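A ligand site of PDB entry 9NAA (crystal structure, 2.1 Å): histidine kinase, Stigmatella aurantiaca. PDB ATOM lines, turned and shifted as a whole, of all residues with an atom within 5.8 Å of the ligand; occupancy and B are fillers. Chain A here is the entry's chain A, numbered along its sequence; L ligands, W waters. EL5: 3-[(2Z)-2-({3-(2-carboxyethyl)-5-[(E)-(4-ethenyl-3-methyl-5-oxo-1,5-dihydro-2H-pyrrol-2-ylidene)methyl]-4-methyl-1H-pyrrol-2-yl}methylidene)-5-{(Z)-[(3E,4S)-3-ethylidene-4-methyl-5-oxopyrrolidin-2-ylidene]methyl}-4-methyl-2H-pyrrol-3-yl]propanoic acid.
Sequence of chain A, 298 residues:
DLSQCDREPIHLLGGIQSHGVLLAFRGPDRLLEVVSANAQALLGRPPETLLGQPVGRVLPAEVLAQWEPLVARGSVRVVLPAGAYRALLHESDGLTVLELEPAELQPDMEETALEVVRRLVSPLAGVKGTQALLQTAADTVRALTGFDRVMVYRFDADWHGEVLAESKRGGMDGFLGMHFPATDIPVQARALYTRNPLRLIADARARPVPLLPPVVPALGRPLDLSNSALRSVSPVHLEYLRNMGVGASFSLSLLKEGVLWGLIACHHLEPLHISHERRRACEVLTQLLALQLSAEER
SG of Cys 5 is covalently linked to CBA of the ligand (1.7 Å). OD1 of Asp 184 sits close to NA of the ligand. An oxygen (O1C) of the ligand lies within hydrogen-bond range of a ring nitrogen (NE2) of His 267 (2.7 Å). NH1 of Arg 231 is in salt-bridge range of O2B of the ligand, 3.0 Å away. O1B of the ligand is in salt-bridge range of NE of Arg 199, 3.3 Å away. A ring nitrogen (ND1) of His 237 is in hydrogen-bond range of a nitrogen (NC) of the ligand (3.3 Å). The side-chain hydroxyl (OH) of Tyr 153 lies close to an oxygen (O2C) of the ligand, 3.5 Å away.
The side-chain carboxylate of Asp 184 sits at hydrogen-bond distance from the backbone NH of Ala 182, 2.9 Å away. The guanidinium group of Arg 199 lies within hydrogen-bond range of the backbone carbonyl oxygen of Arg 231. The backbone NH (N) of Ser 251 sits at hydrogen-bond distance from the backbone carbonyl oxygen (O) of Arg 199 (2.8 Å). The backbone NH (N) of Leu 2 is in hydrogen-bond range of the side-chain carboxylate (OD2) of Asp 6. N of Val 236 lies close to OG of Ser 234, 3.5 Å away. N of Tyr 153 sits at hydrogen-bond distance from O of Leu 263 (2.6 Å). OE2 of Glu 8 lies within hydrogen-bond range of OG of Ser 234 (2.7 Å). The backbone carbonyl oxygen of Ser 249 lies within hydrogen-bond range of the backbone NH of Ile 201 (2.8 Å).
The backbone carbonyl oxygen (O) of Val 236 lies close to an oxygen (OD) of the ligand (3.5 Å). Residues that only touch the ligand: Tyr 193, Ala 265, Leu 2, Asp 6, Ser 234, Pro 186, Tyr 240, Pro 181, Ile 185, Leu 263, Ile 10, Ser 249 and Ala 189. 21 residues have an atom within 4 Å of the ligand: Leu 2, Cys 5, Asp 6, Ile 10, Tyr 153, Pro 181, Asp 184, Ile 185, Pro 186, Ala 189, Tyr 193, Arg 199, Arg 231, Ser 234, Val 236, His 237, Tyr 240, Ser 249, Leu 263, Ala 265 and His 267. The nearest printed residue that does not touch the ligand is Leu 241 (4.1 Å).
Water W4 bridges an oxygen (O2B) of the ligand (2.4 Å) and the backbone NH of Ser 234 (2.9 Å). Water W1 lies within hydrogen-bond range of the side-chain hydroxyl (OH) of Tyr 153 (2.4 Å), an oxygen (O2C) of the ligand (2.6 Å) and the side-chain hydroxyl (OH) of Tyr 240 (3.4 Å). Water W3 lies within hydrogen-bond range of a ring nitrogen (NE2) of His 237 (2.5 Å), an oxygen (O1C) of the ligand (2.9 Å) and the side-chain hydroxyl (OG) of Ser 249 (3.0 Å). Water W2 bridges O of Cys 5 (2.5 Å) and OE2 of Glu 8 (2.7 Å).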
ATOM      1  N   LEU A   2      -0.213  14.752   1.280  1.00  0.00           N
ATOM      2  CA  LEU A   2      -1.164  15.645   0.626  1.00  0.00           C
ATOM      3  C   LEU A   2      -2.533  14.971   0.529  1.00  0.00           C
ATOM      4  O   LEU A   2      -3.189  15.004  -0.516  1.00  0.00           O
ATOM      5  CB  LEU A   2      -0.690  16.087  -0.758  1.00  0.00           C
ATOM      6  CG  LEU A   2       0.647  16.835  -0.870  1.00  0.00           C
ATOM      7  CD1 LEU A   2       1.123  16.863  -2.312  1.00  0.00           C
ATOM      8  CD2 LEU A   2       0.543  18.244  -0.304  1.00  0.00           C
ATOM      9  N   CYS A   5      -5.077  14.406  -2.114  1.00  0.00           N
ATOM     10  CA  CYS A   5      -4.904  13.513  -3.254  1.00  0.00           C
ATOM     11  C   CYS A   5      -4.406  12.118  -2.872  1.00  0.00           C
ATOM     12  O   CYS A   5      -4.339  11.261  -3.757  1.00  0.00           O
ATOM     13  CB  CYS A   5      -3.922  14.105  -4.276  1.00  0.00           C
ATOM     14  SG  CYS A   5      -2.238  14.350  -3.630  1.00  0.00           S
ATOM     15  N   ASP A   6      -4.062  11.878  -1.614  1.00  0.00           N
ATOM     16  CA  ASP A   6      -3.647  10.537  -1.213  1.00  0.00           C
ATOM     17  C   ASP A   6      -4.833   9.634  -0.898  1.00  0.00           C
ATOM     18  O   ASP A   6      -4.640   8.472  -0.505  1.00  0.00           O
ATOM     19  CB  ASP A   6      -2.700  10.602  -0.004  1.00  0.00           C
ATOM     20  CG  ASP A   6      -1.281  11.036  -0.370  1.00  0.00           C
ATOM     21  OD1 ASP A   6      -0.724  10.570  -1.408  1.00  0.00           O
ATOM     22  OD2 ASP A   6      -0.707  11.870   0.373  1.00  0.00           O
ATOM     23  N   GLU A   8      -7.045   9.678  -3.557  1.00  0.00           N
ATOM     24  CA  GLU A   8      -7.550   9.756  -4.937  1.00  0.00           C
ATOM     25  C   GLU A   8      -7.907   8.367  -5.462  1.00  0.00           C
ATOM     26  O   GLU A   8      -7.067   7.459  -5.434  1.00  0.00           O
ATOM     27  CB  GLU A   8      -6.486  10.383  -5.827  1.00  0.00           C
ATOM     28  CG  GLU A   8      -6.988  10.839  -7.184  1.00  0.00           C
ATOM     29  CD  GLU A   8      -5.878  11.376  -8.110  1.00  0.00           C
ATOM     30  OE1 GLU A   8      -6.174  11.606  -9.307  1.00  0.00           O
ATOM     31  OE2 GLU A   8      -4.733  11.636  -7.639  1.00  0.00           O
ATOM     32  N   ILE A  10      -7.661   6.585  -8.128  1.00  0.00           N
ATOM     33  CA  ILE A  10      -7.033   6.604  -9.437  1.00  0.00           C
ATOM     34  C   ILE A  10      -7.518   5.486 -10.345  1.00  0.00           C
ATOM     35  O   ILE A  10      -7.246   5.507 -11.544  1.00  0.00           O
ATOM     36  CB  ILE A  10      -5.503   6.511  -9.279  1.00  0.00           C
ATOM     37  CG1 ILE A  10      -5.179   5.206  -8.532  1.00  0.00           C
ATOM     38  CG2 ILE A  10      -4.977   7.727  -8.536  1.00  0.00           C
ATOM     39  CD1 ILE A  10      -3.714   4.833  -8.546  1.00  0.00           C
ATOM     40  N   TYR A 153      13.668   1.924  -7.786  1.00  0.00           N
ATOM     41  CA  TYR A 153      13.340   2.209  -6.392  1.00  0.00           C
ATOM     42  C   TYR A 153      13.089   0.898  -5.660  1.00  0.00           C
ATOM     43  O   TYR A 153      12.515  -0.032  -6.226  1.00  0.00           O
ATOM     44  CB  TYR A 153      12.087   3.087  -6.285  1.00  0.00           C
ATOM     45  CG  TYR A 153      12.100   4.360  -7.106  1.00  0.00           C
ATOM     46  CD1 TYR A 153      12.625   5.534  -6.609  1.00  0.00           C
ATOM     47  CD2 TYR A 153      11.538   4.380  -8.370  1.00  0.00           C
ATOM     48  CE1 TYR A 153      12.632   6.698  -7.369  1.00  0.00           C
ATOM     49  CE2 TYR A 153      11.532   5.543  -9.134  1.00  0.00           C
ATOM     50  CZ  TYR A 153      12.077   6.707  -8.628  1.00  0.00           C
ATOM     51  OH  TYR A 153      12.070   7.869  -9.392  1.00  0.00           O
ATOM     52  N   PHE A 180      14.084  10.602  -3.329  1.00  0.00           N
ATOM     53  CA  PHE A 180      13.196   9.511  -3.010  1.00  0.00           C
ATOM     54  C   PHE A 180      11.757   9.932  -3.317  1.00  0.00           C
ATOM     55  O   PHE A 180      11.418  11.120  -3.213  1.00  0.00           O
ATOM     56  CB  PHE A 180      13.319   9.135  -1.528  1.00  0.00           C
ATOM     57  CG  PHE A 180      14.685   8.578  -1.133  1.00  0.00           C
ATOM     58  CD1 PHE A 180      15.677   8.324  -2.098  1.00  0.00           C
ATOM     59  CD2 PHE A 180      14.969   8.291   0.207  1.00  0.00           C
ATOM     60  CE1 PHE A 180      16.911   7.814  -1.718  1.00  0.00           C
ATOM     61  CE2 PHE A 180      16.203   7.781   0.587  1.00  0.00           C
ATOM     62  CZ  PHE A 180      17.183   7.542  -0.367  1.00  0.00           C
ATOM     63  N   PRO A 181      10.920   9.026  -3.813  1.00  0.00           N
ATOM     64  CA  PRO A 181       9.477   9.241  -3.749  1.00  0.00           C
ATOM     65  C   PRO A 181       9.022   8.967  -2.335  1.00  0.00           C
ATOM     66  O   PRO A 181       8.666   7.824  -1.997  1.00  0.00           O
ATOM     67  CB  PRO A 181       8.910   8.249  -4.770  1.00  0.00           C
ATOM     68  CG  PRO A 181       9.895   7.164  -4.797  1.00  0.00           C
ATOM     69  CD  PRO A 181      11.243   7.834  -4.607  1.00  0.00           C
ATOM     70  N   ALA A 182       8.961  10.022  -1.522  1.00  0.00           N
ATOM     71  CA  ALA A 182       8.976   9.917  -0.070  1.00  0.00           C
ATOM     72  C   ALA A 182       7.609   9.680   0.542  1.00  0.00           C
ATOM     73  O   ALA A 182       6.996   8.637   0.300  1.00  0.00           O
ATOM     74  CB  ALA A 182       9.551  11.217   0.481  1.00  0.00           C
ATOM     75  N   THR A 183       7.099  10.653   1.308  1.00  0.00           N
ATOM     76  CA  THR A 183       5.712  10.588   1.770  1.00  0.00           C
ATOM     77  C   THR A 183       4.891  10.785   0.499  1.00  0.00           C
ATOM     78  O   THR A 183       4.326  11.854   0.217  1.00  0.00           O
ATOM     79  CB  THR A 183       5.414  11.623   2.861  1.00  0.00           C
ATOM     80  OG1 THR A 183       6.019  12.878   2.517  1.00  0.00           O
ATOM     81  CG2 THR A 183       5.924  11.138   4.220  1.00  0.00           C
ATOM     82  N   ASP A 184       4.830   9.716  -0.303  1.00  0.00           N
ATOM     83  CA  ASP A 184       4.697   9.911  -1.724  1.00  0.00           C
ATOM     84  C   ASP A 184       3.631   9.042  -2.345  1.00  0.00           C
ATOM     85  O   ASP A 184       2.496   9.482  -2.537  1.00  0.00           O
ATOM     86  CB  ASP A 184       6.036   9.629  -2.377  1.00  0.00           C
ATOM     87  CG  ASP A 184       6.337  10.523  -3.594  1.00  0.00           C
ATOM     88  OD1 ASP A 184       5.662  10.373  -4.641  1.00  0.00           O
ATOM     89  OD2 ASP A 184       7.246  11.370  -3.502  1.00  0.00           O
ATOM     90  N   ILE A 185       4.014   7.836  -2.746  1.00  0.00           N
ATOM     91  CA  ILE A 185       3.169   7.069  -3.653  1.00  0.00           C
ATOM     92  C   ILE A 185       2.011   6.525  -2.834  1.00  0.00           C
ATOM     93  O   ILE A 185       2.213   5.700  -1.921  1.00  0.00           O
ATOM     94  CB  ILE A 185       3.979   5.980  -4.386  1.00  0.00           C
ATOM     95  CG1 ILE A 185       5.149   6.631  -5.122  1.00  0.00           C
ATOM     96  CG2 ILE A 185       3.093   5.237  -5.354  1.00  0.00           C
ATOM     97  CD1 ILE A 185       5.974   5.679  -5.900  1.00  0.00           C
ATOM     98  N   PRO A 186       0.795   6.985  -3.100  1.00  0.00           N
ATOM     99  CA  PRO A 186      -0.360   6.609  -2.269  1.00  0.00           C
ATOM    100  C   PRO A 186      -0.652   5.114  -2.375  1.00  0.00           C
ATOM    101  O   PRO A 186      -0.322   4.450  -3.370  1.00  0.00           O
ATOM    102  CB  PRO A 186      -1.505   7.440  -2.864  1.00  0.00           C
ATOM    103  CG  PRO A 186      -1.107   7.617  -4.291  1.00  0.00           C
ATOM    104  CD  PRO A 186       0.390   7.744  -4.296  1.00  0.00           C
ATOM    105  N   ALA A 189      -2.079   3.656  -5.556  1.00  0.00           N
ATOM    106  CA  ALA A 189      -1.127   3.504  -6.645  1.00  0.00           C
ATOM    107  C   ALA A 189      -0.273   2.251  -6.444  1.00  0.00           C
ATOM    108  O   ALA A 189      -0.097   1.470  -7.381  1.00  0.00           O
ATOM    109  CB  ALA A 189      -0.253   4.750  -6.782  1.00  0.00           C
ATOM    110  N   TYR A 193       0.138  -1.090  -8.825  1.00  0.00           N
ATOM    111  CA  TYR A 193       1.449  -1.581  -9.220  1.00  0.00           C
ATOM    112  C   TYR A 193       1.627  -3.059  -8.847  1.00  0.00           C
ATOM    113  O   TYR A 193       2.366  -3.793  -9.527  1.00  0.00           O
ATOM    114  CB  TYR A 193       2.522  -0.764  -8.518  1.00  0.00           C
ATOM    115  CG  TYR A 193       2.550   0.696  -8.882  1.00  0.00           C
ATOM    116  CD1 TYR A 193       3.400   1.555  -8.213  1.00  0.00           C
ATOM    117  CD2 TYR A 193       1.691   1.222  -9.857  1.00  0.00           C
ATOM    118  CE1 TYR A 193       3.441   2.872  -8.501  1.00  0.00           C
ATOM    119  CE2 TYR A 193       1.706   2.569 -10.136  1.00  0.00           C
ATOM    120  CZ  TYR A 193       2.601   3.379  -9.461  1.00  0.00           C
ATOM    121  OH  TYR A 193       2.684   4.713  -9.720  1.00  0.00           O
ATOM    122  N   ARG A 199       3.343  -0.566 -16.671  1.00  0.00           N
ATOM    123  CA  ARG A 199       2.516   0.641 -16.738  1.00  0.00           C
ATOM    124  C   ARG A 199       3.150   1.644 -17.711  1.00  0.00           C
ATOM    125  O   ARG A 199       4.322   1.991 -17.550  1.00  0.00           O
ATOM    126  CB  ARG A 199       2.340   1.214 -15.329  1.00  0.00           C
ATOM    127  CG  ARG A 199       1.742   2.579 -15.276  1.00  0.00           C
ATOM    128  CD  ARG A 199       0.339   2.494 -15.829  1.00  0.00           C
ATOM    129  NE  ARG A 199      -0.474   3.663 -15.538  1.00  0.00           N
ATOM    130  CZ  ARG A 199      -1.500   4.023 -16.291  1.00  0.00           C
ATOM    131  NH1 ARG A 199      -1.812   3.366 -17.394  1.00  0.00           N
ATOM    132  NH2 ARG A 199      -2.226   5.080 -15.932  1.00  0.00           N
ATOM    133  N   ILE A 201       2.745   5.435 -19.594  1.00  0.00           N
ATOM    134  CA  ILE A 201       2.195   6.754 -19.893  1.00  0.00           C
ATOM    135  C   ILE A 201       2.859   7.197 -21.196  1.00  0.00           C
ATOM    136  O   ILE A 201       4.029   7.553 -21.216  1.00  0.00           O
ATOM    137  CB  ILE A 201       2.454   7.756 -18.772  1.00  0.00           C
ATOM    138  CG1 ILE A 201       2.019   7.188 -17.420  1.00  0.00           C
ATOM    139  CG2 ILE A 201       1.764   9.080 -19.076  1.00  0.00           C
ATOM    140  CD1 ILE A 201       2.469   8.012 -16.240  1.00  0.00           C
ATOM    141  N   ARG A 231      -5.375   3.288 -19.045  1.00  0.00           N
ATOM    142  CA  ARG A 231      -5.864   4.089 -17.924  1.00  0.00           C
ATOM    143  C   ARG A 231      -5.149   5.431 -17.859  1.00  0.00           C
ATOM    144  O   ARG A 231      -3.914   5.493 -17.870  1.00  0.00           O
ATOM    145  CB  ARG A 231      -5.662   3.322 -16.602  1.00  0.00           C
ATOM    146  CG  ARG A 231      -6.095   4.125 -15.332  1.00  0.00           C
ATOM    147  CD  ARG A 231      -5.844   3.380 -14.004  1.00  0.00           C
ATOM    148  NE  ARG A 231      -4.564   2.665 -13.966  1.00  0.00           N
ATOM    149  CZ  ARG A 231      -3.445   3.141 -13.427  1.00  0.00           C
ATOM    150  NH1 ARG A 231      -3.408   4.303 -12.798  1.00  0.00           N
ATOM    151  NH2 ARG A 231      -2.330   2.412 -13.521  1.00  0.00           N
ATOM    152  N   SER A 232      -5.942   6.499 -17.827  1.00  0.00           N
ATOM    153  CA  SER A 232      -5.377   7.827 -17.686  1.00  0.00           C
ATOM    154  C   SER A 232      -4.749   7.972 -16.307  1.00  0.00           C
ATOM    155  O   SER A 232      -4.980   7.176 -15.394  1.00  0.00           O
ATOM    156  CB  SER A 232      -6.462   8.893 -17.879  1.00  0.00           C
ATOM    157  OG  SER A 232      -7.433   8.797 -16.830  1.00  0.00           O
ATOM    158  N   VAL A 233      -3.991   9.033 -16.126  1.00  0.00           N
ATOM    159  CA  VAL A 233      -3.130   9.130 -14.952  1.00  0.00           C
ATOM    160  C   VAL A 233      -3.564  10.294 -14.085  1.00  0.00           C
ATOM    161  O   VAL A 233      -4.091  11.309 -14.572  1.00  0.00           O
ATOM    162  CB  VAL A 233      -1.648   9.214 -15.368  1.00  0.00           C
ATOM    163  CG1 VAL A 233      -1.515   9.440 -16.861  1.00  0.00           C
ATOM    164  CG2 VAL A 233      -0.879  10.215 -14.517  1.00  0.00           C
ATOM    165  N   SER A 234      -3.417  10.107 -12.753  1.00  0.00           N
ATOM    166  CA  SER A 234      -3.669  11.148 -11.760  1.00  0.00           C
ATOM    167  C   SER A 234      -3.051  12.468 -12.223  1.00  0.00           C
ATOM    168  O   SER A 234      -1.847  12.513 -12.507  1.00  0.00           O
ATOM    169  CB  SER A 234      -3.099  10.735 -10.413  1.00  0.00           C
ATOM    170  OG  SER A 234      -2.858  11.858  -9.581  1.00  0.00           O
ATOM    171  N   VAL A 236      -2.019  15.032 -10.652  1.00  0.00           N
ATOM    172  CA  VAL A 236      -0.894  15.474  -9.826  1.00  0.00           C
ATOM    173  C   VAL A 236       0.404  14.803 -10.291  1.00  0.00           C
ATOM    174  O   VAL A 236       1.454  15.452 -10.350  1.00  0.00           O
ATOM    175  CB  VAL A 236      -1.184  15.181  -8.342  1.00  0.00           C
ATOM    176  CG1 VAL A 236      -0.053  15.700  -7.478  1.00  0.00           C
ATOM    177  CG2 VAL A 236      -2.511  15.802  -7.920  1.00  0.00           C
ATOM    178  N   HIS A 237       0.344  13.518 -10.644  1.00  0.00           N
ATOM    179  CA  HIS A 237       1.553  12.873 -11.136  1.00  0.00           C
ATOM    180  C   HIS A 237       1.874  13.278 -12.570  1.00  0.00           C
ATOM    181  O   HIS A 237       3.051  13.337 -12.933  1.00  0.00           O
ATOM    182  CB  HIS A 237       1.416  11.350 -11.026  1.00  0.00           C
ATOM    183  CG  HIS A 237       2.611  10.599 -11.528  1.00  0.00           C
ATOM    184  ND1 HIS A 237       3.855  10.682 -10.947  1.00  0.00           N
ATOM    185  CD2 HIS A 237       2.740   9.715 -12.555  1.00  0.00           C
ATOM    186  CE1 HIS A 237       4.715   9.922 -11.607  1.00  0.00           C
ATOM    187  NE2 HIS A 237       4.055   9.312 -12.582  1.00  0.00           N
ATOM    188  N   TYR A 240       3.780  16.354 -12.319  1.00  0.00           N
ATOM    189  CA  TYR A 240       5.150  16.150 -11.853  1.00  0.00           C
ATOM    190  C   TYR A 240       6.054  15.709 -13.004  1.00  0.00           C
ATOM    191  O   TYR A 240       7.208  16.162 -13.103  1.00  0.00           O
ATOM    192  CB  TYR A 240       5.156  15.135 -10.692  1.00  0.00           C
ATOM    193  CG  TYR A 240       6.445  14.352 -10.533  1.00  0.00           C
ATOM    194  CD1 TYR A 240       7.490  14.837  -9.741  1.00  0.00           C
ATOM    195  CD2 TYR A 240       6.618  13.122 -11.159  1.00  0.00           C
ATOM    196  CE1 TYR A 240       8.679  14.117  -9.603  1.00  0.00           C
ATOM    197  CE2 TYR A 240       7.799  12.398 -11.041  1.00  0.00           C
ATOM    198  CZ  TYR A 240       8.829  12.900 -10.251  1.00  0.00           C
ATOM    199  OH  TYR A 240       9.994  12.169 -10.130  1.00  0.00           O
ATOM    200  N   LEU A 241       5.563  14.845 -13.887  1.00  0.00           N
ATOM    201  CA  LEU A 241       6.338  14.460 -15.059  1.00  0.00           C
ATOM    202  C   LEU A 241       6.580  15.662 -15.977  1.00  0.00           C
ATOM    203  O   LEU A 241       7.708  15.861 -16.488  1.00  0.00           O
ATOM    204  CB  LEU A 241       5.624  13.332 -15.807  1.00  0.00           C
ATOM    205  CG  LEU A 241       5.476  11.988 -15.066  1.00  0.00           C
ATOM    206  CD1 LEU A 241       4.676  11.019 -15.921  1.00  0.00           C
ATOM    207  CD2 LEU A 241       6.829  11.372 -14.646  1.00  0.00           C
ATOM    208  N   SER A 249       6.787   7.782 -20.020  1.00  0.00           N
ATOM    209  CA  SER A 249       7.147   7.161 -18.754  1.00  0.00           C
ATOM    210  C   SER A 249       6.683   5.713 -18.771  1.00  0.00           C
ATOM    211  O   SER A 249       5.515   5.427 -19.072  1.00  0.00           O
ATOM    212  CB  SER A 249       6.547   7.951 -17.587  1.00  0.00           C
ATOM    213  OG  SER A 249       6.666   7.294 -16.349  1.00  0.00           O
ATOM    214  N   SER A 251       6.989   2.035 -16.554  1.00  0.00           N
ATOM    215  CA  SER A 251       7.281   1.549 -15.211  1.00  0.00           C
ATOM    216  C   SER A 251       7.086   0.042 -15.129  1.00  0.00           C
ATOM    217  O   SER A 251       6.195  -0.511 -15.789  1.00  0.00           O
ATOM    218  CB  SER A 251       6.386   2.235 -14.172  1.00  0.00           C
ATOM    219  OG  SER A 251       6.441   3.649 -14.357  1.00  0.00           O
ATOM    220  N   LEU A 263      10.289  -0.661  -7.788  1.00  0.00           N
ATOM    221  CA  LEU A 263       9.740  -0.106  -9.012  1.00  0.00           C
ATOM    222  C   LEU A 263      10.908   0.319  -9.892  1.00  0.00           C
ATOM    223  O   LEU A 263      11.851   0.932  -9.405  1.00  0.00           O
ATOM    224  CB  LEU A 263       8.824   1.071  -8.683  1.00  0.00           C
ATOM    225  CG  LEU A 263       7.766   1.432  -9.705  1.00  0.00           C
ATOM    226  CD1 LEU A 263       6.791   0.273  -9.798  1.00  0.00           C
ATOM    227  CD2 LEU A 263       7.071   2.682  -9.243  1.00  0.00           C
ATOM    228  N   ALA A 265      11.530   2.746 -12.976  1.00  0.00           N
ATOM    229  CA  ALA A 265      10.871   3.865 -13.669  1.00  0.00           C
ATOM    230  C   ALA A 265      11.731   4.353 -14.829  1.00  0.00           C
ATOM    231  O   ALA A 265      12.851   4.835 -14.617  1.00  0.00           O
ATOM    232  CB  ALA A 265      10.602   5.012 -12.688  1.00  0.00           C
ATOM    233  N   HIS A 267      12.084   7.066 -17.883  1.00  0.00           N
ATOM    234  CA  HIS A 267      11.650   8.386 -18.311  1.00  0.00           C
ATOM    235  C   HIS A 267      12.390   8.738 -19.584  1.00  0.00           C
ATOM    236  O   HIS A 267      13.598   8.539 -19.679  1.00  0.00           O
ATOM    237  CB  HIS A 267      11.903   9.439 -17.227  1.00  0.00           C
ATOM    238  CG  HIS A 267      11.036   9.269 -16.005  1.00  0.00           C
ATOM    239  ND1 HIS A 267      11.311   9.892 -14.802  1.00  0.00           N
ATOM    240  CD2 HIS A 267       9.923   8.536 -15.803  1.00  0.00           C
ATOM    241  CE1 HIS A 267      10.398   9.544 -13.921  1.00  0.00           C
ATOM    242  NE2 HIS A 267       9.547   8.718 -14.498  1.00  0.00           N
HETATM  243  C1A EL5 L   1       3.070  12.014  -4.582  1.00  0.00           C
HETATM  244  C1B EL5 L   1       1.141   9.371  -7.565  1.00  0.00           C
HETATM  245  O1B EL5 L   1       1.025   5.456 -13.261  1.00  0.00           O
HETATM  246  C1C EL5 L   1       5.196   8.161  -8.753  1.00  0.00           C
HETATM  247  O1C EL5 L   1       7.725   7.900 -12.655  1.00  0.00           O
HETATM  248  C1D EL5 L   1       6.397  12.053  -7.381  1.00  0.00           C
HETATM  249  C2A EL5 L   1       1.794  12.535  -4.002  1.00  0.00           C
HETATM  250  C2B EL5 L   1       0.343   8.491  -8.417  1.00  0.00           C
HETATM  251  O2B EL5 L   1      -0.984   6.067 -12.613  1.00  0.00           O
HETATM  252  C2C EL5 L   1       6.503   7.714  -8.886  1.00  0.00           C
HETATM  253  O2C EL5 L   1       8.956   7.432 -10.925  1.00  0.00           O
HETATM  254  C2D EL5 L   1       6.674  13.309  -6.636  1.00  0.00           C
HETATM  255  C3A EL5 L   1       0.648  11.903  -4.781  1.00  0.00           C
HETATM  256  C3B EL5 L   1       1.258   7.651  -9.143  1.00  0.00           C
HETATM  257  C3C EL5 L   1       7.332   8.680  -8.447  1.00  0.00           C
HETATM  258  C3D EL5 L   1       5.546  14.189  -6.711  1.00  0.00           C
HETATM  259  C4A EL5 L   1       1.193  11.015  -5.830  1.00  0.00           C
HETATM  260  C4B EL5 L   1       2.723   7.991  -8.735  1.00  0.00           C
HETATM  261  C4C EL5 L   1       6.592   9.729  -8.042  1.00  0.00           C
HETATM  262  C4D EL5 L   1       4.454  13.576  -7.543  1.00  0.00           C
HETATM  263  CAA EL5 L   1      -0.653  12.033  -4.593  1.00  0.00           C
HETATM  264  CAB EL5 L   1       0.724   6.624 -10.146  1.00  0.00           C
HETATM  265  CAC EL5 L   1       6.953   6.364  -9.429  1.00  0.00           C
HETATM  266  CAD EL5 L   1       5.485  15.567  -6.063  1.00  0.00           C
HETATM  267  CBA EL5 L   1      -1.382  13.331  -4.657  1.00  0.00           C
HETATM  268  CBB EL5 L   1       0.817   7.195 -11.544  1.00  0.00           C
HETATM  269  CBC EL5 L   1       6.765   6.420 -10.935  1.00  0.00           C
HETATM  270  CBD EL5 L   1       4.634  16.479  -6.496  1.00  0.00           C
HETATM  271  CGB EL5 L   1       0.263   6.163 -12.528  1.00  0.00           C
HETATM  272  CGC EL5 L   1       7.868   7.310 -11.546  1.00  0.00           C
HETATM  273  CHB EL5 L   1       0.476  10.357  -6.666  1.00  0.00           C
HETATM  274  CHC EL5 L   1       3.874   7.467  -9.134  1.00  0.00           C
HETATM  275  CHD EL5 L   1       7.189  11.025  -7.489  1.00  0.00           C
HETATM  276  CMA EL5 L   1       1.855  14.042  -4.221  1.00  0.00           C
HETATM  277  CMB EL5 L   1      -1.188   8.471  -8.530  1.00  0.00           C
HETATM  278  CMC EL5 L   1       8.849   8.716  -8.336  1.00  0.00           C
HETATM  279  CMD EL5 L   1       7.959  13.597  -5.864  1.00  0.00           C
HETATM  280  NA  EL5 L   1       2.723  11.068  -5.742  1.00  0.00           N
HETATM  281  OA  EL5 L   1       4.150  12.324  -4.222  1.00  0.00           O
HETATM  282  NB  EL5 L   1       2.581   9.117  -7.727  1.00  0.00           N
HETATM  283  NC  EL5 L   1       5.287   9.390  -8.231  1.00  0.00           N
HETATM  284  ND  EL5 L   1       4.977  12.195  -7.982  1.00  0.00           N
HETATM  285  OD  EL5 L   1       3.402  14.059  -7.814  1.00  0.00           O
HETATM  286  O   HOH W   1      10.958   9.088 -11.167  1.00  0.00           O
HETATM  287  O   HOH W   2      -3.355  10.223  -5.757  1.00  0.00           O
HETATM  288  O   HOH W   3       5.134   7.475 -13.802  1.00  0.00           O
HETATM  289  O   HOH W   4      -2.575   7.573 -11.549  1.00  0.00           O
HETATM  290  O   HOH W   5       3.464   5.403 -13.094  1.00  0.00           O
